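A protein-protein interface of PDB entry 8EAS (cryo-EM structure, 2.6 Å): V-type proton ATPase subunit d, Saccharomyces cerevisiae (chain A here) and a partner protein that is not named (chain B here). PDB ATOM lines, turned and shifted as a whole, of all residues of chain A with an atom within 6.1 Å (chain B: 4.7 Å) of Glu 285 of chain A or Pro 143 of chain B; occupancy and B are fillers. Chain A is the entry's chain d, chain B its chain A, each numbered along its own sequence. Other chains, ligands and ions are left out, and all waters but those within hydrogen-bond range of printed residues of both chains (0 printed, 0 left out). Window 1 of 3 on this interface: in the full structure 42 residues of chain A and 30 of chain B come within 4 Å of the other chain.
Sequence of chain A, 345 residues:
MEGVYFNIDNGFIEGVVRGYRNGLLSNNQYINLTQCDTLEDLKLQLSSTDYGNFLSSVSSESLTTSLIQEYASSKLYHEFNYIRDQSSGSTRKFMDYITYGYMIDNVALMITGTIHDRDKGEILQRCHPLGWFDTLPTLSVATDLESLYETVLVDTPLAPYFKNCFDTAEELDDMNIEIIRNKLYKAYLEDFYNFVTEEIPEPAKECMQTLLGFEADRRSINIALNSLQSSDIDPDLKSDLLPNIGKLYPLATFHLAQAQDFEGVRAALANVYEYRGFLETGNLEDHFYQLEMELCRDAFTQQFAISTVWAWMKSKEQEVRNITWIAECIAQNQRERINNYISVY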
ATOM      1  N   ASN A 222      19.443  13.461  10.096  1.00  0.00           N
ATOM      2  CA  ASN A 222      20.869  13.182  10.220  1.00  0.00           C
ATOM      3  C   ASN A 222      21.158  11.698  10.038  1.00  0.00           C
ATOM      4  O   ASN A 222      22.100  11.324   9.336  1.00  0.00           O
ATOM      5  CB  ASN A 222      21.383  13.666  11.572  1.00  0.00           C
ATOM      6  CG  ASN A 222      21.647  15.146  11.587  1.00  0.00           C
ATOM      7  OD1 ASN A 222      21.667  15.791  10.543  1.00  0.00           O
ATOM      8  ND2 ASN A 222      21.852  15.697  12.774  1.00  0.00           N
ATOM      9  N   ASN A 283      23.597  24.795   4.235  1.00  0.00           N
ATOM     10  CA  ASN A 283      24.053  23.677   5.046  1.00  0.00           C
ATOM     11  C   ASN A 283      22.870  23.118   5.824  1.00  0.00           C
ATOM     12  O   ASN A 283      22.021  23.870   6.306  1.00  0.00           O
ATOM     13  CB  ASN A 283      25.165  24.117   6.002  1.00  0.00           C
ATOM     14  CG  ASN A 283      25.802  22.953   6.745  1.00  0.00           C
ATOM     15  OD1 ASN A 283      25.293  21.833   6.737  1.00  0.00           O
ATOM     16  ND2 ASN A 283      26.922  23.220   7.399  1.00  0.00           N
ATOM     17  N   LEU A 284      22.813  21.790   5.929  1.00  0.00           N
ATOM     18  CA  LEU A 284      21.707  21.158   6.638  1.00  0.00           C
ATOM     19  C   LEU A 284      21.696  21.552   8.107  1.00  0.00           C
ATOM     20  O   LEU A 284      20.631  21.779   8.690  1.00  0.00           O
ATOM     21  CB  LEU A 284      21.788  19.641   6.500  1.00  0.00           C
ATOM     22  CG  LEU A 284      20.683  18.912   7.265  1.00  0.00           C
ATOM     23  CD1 LEU A 284      19.404  18.888   6.453  1.00  0.00           C
ATOM     24  CD2 LEU A 284      21.109  17.513   7.664  1.00  0.00           C
ATOM     25  N   GLU A 285      22.872  21.625   8.726  1.00  0.00           N
ATOM     26  CA  GLU A 285      22.947  21.932  10.146  1.00  0.00           C
ATOM     27  C   GLU A 285      22.630  23.391  10.434  1.00  0.00           C
ATOM     28  O   GLU A 285      22.084  23.701  11.498  1.00  0.00           O
ATOM     29  CB  GLU A 285      24.327  21.557  10.676  1.00  0.00           C
ATOM     30  CG  GLU A 285      24.499  20.063  10.831  1.00  0.00           C
ATOM     31  CD  GLU A 285      25.938  19.615  10.731  1.00  0.00           C
ATOM     32  OE1 GLU A 285      26.701  20.209   9.940  1.00  0.00           O
ATOM     33  OE2 GLU A 285      26.301  18.653  11.438  1.00  0.00           O
ATOM     34  N   ASP A 286      22.949  24.294   9.507  1.00  0.00           N
ATOM     35  CA  ASP A 286      22.541  25.683   9.674  1.00  0.00           C
ATOM     36  C   ASP A 286      21.029  25.820   9.679  1.00  0.00           C
ATOM     37  O   ASP A 286      20.482  26.608  10.453  1.00  0.00           O
ATOM     38  CB  ASP A 286      23.142  26.549   8.572  1.00  0.00           C
ATOM     39  CG  ASP A 286      24.468  27.137   8.961  1.00  0.00           C
ATOM     40  OD1 ASP A 286      24.909  26.894  10.100  1.00  0.00           O
ATOM     41  OD2 ASP A 286      25.073  27.844   8.130  1.00  0.00           O
ATOM     42  N   HIS A 287      20.339  25.071   8.816  1.00  0.00           N
ATOM     43  CA  HIS A 287      18.883  25.125   8.795  1.00  0.00           C
ATOM     44  C   HIS A 287      18.290  24.630  10.102  1.00  0.00           C
ATOM     45  O   HIS A 287      17.346  25.229  10.625  1.00  0.00           O
ATOM     46  CB  HIS A 287      18.342  24.314   7.622  1.00  0.00           C
ATOM     47  CG  HIS A 287      18.572  24.957   6.292  1.00  0.00           C
ATOM     48  ND1 HIS A 287      19.708  24.735   5.545  1.00  0.00           N
ATOM     49  CD2 HIS A 287      17.819  25.829   5.583  1.00  0.00           C
ATOM     50  CE1 HIS A 287      19.640  25.435   4.428  1.00  0.00           C
ATOM     51  NE2 HIS A 287      18.504  26.109   4.426  1.00  0.00           N
ATOM     52  N   PHE A 288      18.831  23.545  10.649  1.00  0.00           N
ATOM     53  CA  PHE A 288      18.316  23.026  11.909  1.00  0.00           C
ATOM     54  C   PHE A 288      18.615  23.971  13.062  1.00  0.00           C
ATOM     55  O   PHE A 288      17.774  24.161  13.943  1.00  0.00           O
ATOM     56  CB  PHE A 288      18.894  21.643  12.171  1.00  0.00           C
ATOM     57  CG  PHE A 288      18.207  20.562  11.404  1.00  0.00           C
ATOM     58  CD1 PHE A 288      16.830  20.451  11.431  1.00  0.00           C
ATOM     59  CD2 PHE A 288      18.932  19.669  10.642  1.00  0.00           C
ATOM     60  CE1 PHE A 288      16.193  19.469  10.718  1.00  0.00           C
ATOM     61  CE2 PHE A 288      18.297  18.683   9.932  1.00  0.00           C
ATOM     62  CZ  PHE A 288      16.928  18.584   9.970  1.00  0.00           C
ATOM     63  N   TYR A 289      19.801  24.577  13.078  1.00  0.00           N
ATOM     64  CA  TYR A 289      20.114  25.535  14.132  1.00  0.00           C
ATOM     65  C   TYR A 289      19.216  26.763  14.050  1.00  0.00           C
ATOM     66  O   TYR A 289      18.706  27.239  15.074  1.00  0.00           O
ATOM     67  CB  TYR A 289      21.588  25.928  14.062  1.00  0.00           C
ATOM     68  CG  TYR A 289      22.485  24.895  14.683  1.00  0.00           C
ATOM     69  CD1 TYR A 289      22.014  23.626  14.935  1.00  0.00           C
ATOM     70  CD2 TYR A 289      23.788  25.190  15.040  1.00  0.00           C
ATOM     71  CE1 TYR A 289      22.802  22.677  15.501  1.00  0.00           C
ATOM     72  CE2 TYR A 289      24.589  24.234  15.626  1.00  0.00           C
ATOM     73  CZ  TYR A 289      24.082  22.979  15.851  1.00  0.00           C
ATOM     74  OH  TYR A 289      24.834  21.993  16.429  1.00  0.00           O
ATOM     75  N   GLN A 290      18.993  27.274  12.838  1.00  0.00           N
ATOM     76  CA  GLN A 290      18.112  28.420  12.667  1.00  0.00           C
ATOM     77  C   GLN A 290      16.684  28.081  13.062  1.00  0.00           C
ATOM     78  O   GLN A 290      16.008  28.885  13.708  1.00  0.00           O
ATOM     79  CB  GLN A 290      18.171  28.913  11.225  1.00  0.00           C
ATOM     80  CG  GLN A 290      17.345  30.155  10.973  1.00  0.00           C
ATOM     81  CD  GLN A 290      17.855  31.353  11.740  1.00  0.00           C
ATOM     82  OE1 GLN A 290      19.051  31.635  11.751  1.00  0.00           O
ATOM     83  NE2 GLN A 290      16.948  32.063  12.393  1.00  0.00           N
ATOM     84  N   SER B  48      33.355  22.418  13.438  1.00  0.00           N
ATOM     85  CA  SER B  48      32.803  21.162  13.924  1.00  0.00           C
ATOM     86  C   SER B  48      32.469  21.239  15.404  1.00  0.00           C
ATOM     87  O   SER B  48      31.559  20.546  15.865  1.00  0.00           O
ATOM     88  CB  SER B  48      33.788  20.027  13.680  1.00  0.00           C
ATOM     89  OG  SER B  48      34.064  19.904  12.308  1.00  0.00           O
ATOM     90  N   TYR B  51      28.118  23.195  15.567  1.00  0.00           N
ATOM     91  CA  TYR B  51      27.482  21.963  15.085  1.00  0.00           C
ATOM     92  C   TYR B  51      27.890  20.770  15.945  1.00  0.00           C
ATOM     93  O   TYR B  51      28.246  19.713  15.428  1.00  0.00           O
ATOM     94  CB  TYR B  51      27.793  21.653  13.614  1.00  0.00           C
ATOM     95  CG  TYR B  51      27.574  22.757  12.622  1.00  0.00           C
ATOM     96  CD1 TYR B  51      26.415  23.509  12.630  1.00  0.00           C
ATOM     97  CD2 TYR B  51      28.518  23.020  11.646  1.00  0.00           C
ATOM     98  CE1 TYR B  51      26.217  24.506  11.711  1.00  0.00           C
ATOM     99  CE2 TYR B  51      28.328  24.012  10.727  1.00  0.00           C
ATOM    100  CZ  TYR B  51      27.176  24.749  10.760  1.00  0.00           C
ATOM    101  OH  TYR B  51      26.991  25.744   9.834  1.00  0.00           O
ATOM    102  N   TYR B  60      34.678  18.191  19.502  1.00  0.00           N
ATOM    103  CA  TYR B  60      35.304  17.103  18.755  1.00  0.00           C
ATOM    104  C   TYR B  60      36.799  17.180  19.021  1.00  0.00           C
ATOM    105  O   TYR B  60      37.516  17.958  18.391  1.00  0.00           O
ATOM    106  CB  TYR B  60      34.984  17.195  17.268  1.00  0.00           C
ATOM    107  CG  TYR B  60      33.558  16.822  16.967  1.00  0.00           C
ATOM    108  CD1 TYR B  60      33.166  15.497  16.903  1.00  0.00           C
ATOM    109  CD2 TYR B  60      32.597  17.796  16.767  1.00  0.00           C
ATOM    110  CE1 TYR B  60      31.864  15.157  16.644  1.00  0.00           C
ATOM    111  CE2 TYR B  60      31.295  17.465  16.509  1.00  0.00           C
ATOM    112  CZ  TYR B  60      30.932  16.145  16.446  1.00  0.00           C
ATOM    113  OH  TYR B  60      29.628  15.817  16.181  1.00  0.00           O
ATOM    114  N   SER B 141      27.484  10.628  13.816  1.00  0.00           N
ATOM    115  CA  SER B 141      27.517  11.692  14.812  1.00  0.00           C
ATOM    116  C   SER B 141      28.635  12.687  14.543  1.00  0.00           C
ATOM    117  O   SER B 141      29.269  13.191  15.473  1.00  0.00           O
ATOM    118  CB  SER B 141      27.652  11.109  16.216  1.00  0.00           C
ATOM    119  OG  SER B 141      26.716  10.072  16.434  1.00  0.00           O
ATOM    120  N   VAL B 142      28.895  13.003  13.280  1.00  0.00           N
ATOM    121  CA  VAL B 142      29.847  14.065  12.966  1.00  0.00           C
ATOM    122  C   VAL B 142      29.227  15.029  11.965  1.00  0.00           C
ATOM    123  O   VAL B 142      28.395  14.625  11.142  1.00  0.00           O
ATOM    124  CB  VAL B 142      31.173  13.514  12.419  1.00  0.00           C
ATOM    125  CG1 VAL B 142      31.919  12.759  13.489  1.00  0.00           C
ATOM    126  CG2 VAL B 142      30.933  12.652  11.215  1.00  0.00           C
ATOM    127  N   PRO B 143      29.593  16.303  12.010  1.00  0.00           N
ATOM    128  CA  PRO B 143      29.205  17.222  10.942  1.00  0.00           C
ATOM    129  C   PRO B 143      30.065  17.019   9.705  1.00  0.00           C
ATOM    130  O   PRO B 143      31.138  16.415   9.747  1.00  0.00           O
ATOM    131  CB  PRO B 143      29.448  18.598  11.566  1.00  0.00           C
ATOM    132  CG  PRO B 143      30.517  18.367  12.557  1.00  0.00           C
ATOM    133  CD  PRO B 143      30.327  16.983  13.089  1.00  0.00           C
ATOM    134  N   SER B 144      29.564  17.529   8.582  1.00  0.00           N
ATOM    135  CA  SER B 144      30.350  17.498   7.355  1.00  0.00           C
ATOM    136  C   SER B 144      31.603  18.351   7.467  1.00  0.00           C
ATOM    137  O   SER B 144      32.592  18.084   6.773  1.00  0.00           O
ATOM    138  CB  SER B 144      29.494  17.959   6.177  1.00  0.00           C
ATOM    139  OG  SER B 144      28.965  19.252   6.405  1.00  0.00           O
ATOM    140  N   SER B 145      31.586  19.362   8.336  1.00  0.00           N
ATOM    141  CA  SER B 145      32.763  20.197   8.533  1.00  0.00           C
ATOM    142  C   SER B 145      33.913  19.403   9.136  1.00  0.00           C
ATOM    143  O   SER B 145      35.080  19.705   8.878  1.00  0.00           O
ATOM    144  CB  SER B 145      32.409  21.399   9.404  1.00  0.00           C
ATOM    145  OG  SER B 145      31.977  20.985  10.682  1.00  0.00           O
ATOM    146  N   LEU B 146      33.610  18.379   9.934  1.00  0.00           N
ATOM    147  CA  LEU B 146      34.677  17.529  10.454  1.00  0.00           C
ATOM    148  C   LEU B 146      35.325  16.712   9.346  1.00  0.00           C
ATOM    149  O   LEU B 146      36.546  16.516   9.345  1.00  0.00           O
ATOM    150  CB  LEU B 146      34.143  16.619  11.556  1.00  0.00           C
ATOM    151  CG  LEU B 146      35.233  15.903  12.348  1.00  0.00           C
ATOM    152  CD1 LEU B 146      36.230  16.892  12.896  1.00  0.00           C
ATOM    153  CD2 LEU B 146      34.622  15.120  13.468  1.00  0.00           C
ATOM    154  N   ARG B 147      34.527  16.227   8.395  1.00  0.00           N
ATOM    155  CA  ARG B 147      35.093  15.545   7.237  1.00  0.00           C
ATOM    156  C   ARG B 147      35.931  16.497   6.396  1.00  0.00           C
ATOM    157  O   ARG B 147      36.992  16.117   5.888  1.00  0.00           O
ATOM    158  CB  ARG B 147      33.976  14.921   6.409  1.00  0.00           C
ATOM    159  CG  ARG B 147      33.068  14.023   7.222  1.00  0.00           C
ATOM    160  CD  ARG B 147      32.004  13.377   6.362  1.00  0.00           C
ATOM    161  NE  ARG B 147      30.953  12.769   7.167  1.00  0.00           N
ATOM    162  CZ  ARG B 147      31.062  11.597   7.777  1.00  0.00           C
ATOM    163  NH1 ARG B 147      32.163  10.870   7.683  1.00  0.00           N
ATOM    164  NH2 ARG B 147      30.042  11.142   8.496  1.00  0.00           N
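The backbone NH (N) of Glu 285 of chain A is in hydrogen-bond range of the side-chain amide oxygen (OD1) of Asn 283 of chain A (3.1 Å).
ND1 of His 287 of chain A sits at hydrogen-bond distance from O of Asn 283 of chain A.
Of the printed residues of chain B, Asn 283 of chain A touches Tyr 51.
Of chain B, only Tyr 51 and Pro 143 come within 4 Å of Glu 285 of chain A.
Of the printed residues of chain B, Tyr 289 of chain A touches Tyr 51 (3.0 Å).
Printed residues of chain A within 4 Å of Tyr 51 of chain B: Asn 283 (3.5 Å), Glu 285 (3.5 Å), Asp 286 (2.4 Å) and Tyr 289 (3.0 Å).
Pro 143 of chain B touches one residue of chain A.
The nearest printed residue of chain A that does not touch Pro 143 of chain B is Asn 283 of chain A (6.7 Å).
The nearest printed residue of chain B that does not touch Asp 286 of chain A is Ser 144 of chain B (8.4 Å).
Among the printed residues, merely in contact across the chains: Tyr 289 of chain A with Tyr 51 of chain B, Glu 285 of chain A with Pro 143 of chain B, Glu 285 of chain A with Tyr 51 of chain B and Asn 283 of chain A with Tyr 51 of chain B.
Of the 10 printed residues of chain B, 2 touch a printed residue of chain A.
Hydrophobic or aromatic side chains of chain A within 4 Å of the printed part of chain B: Tyr 289.
OH of Tyr 51 of chain B lies close to OD2 of Asp 286 of chain A, at 3.3 Å.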
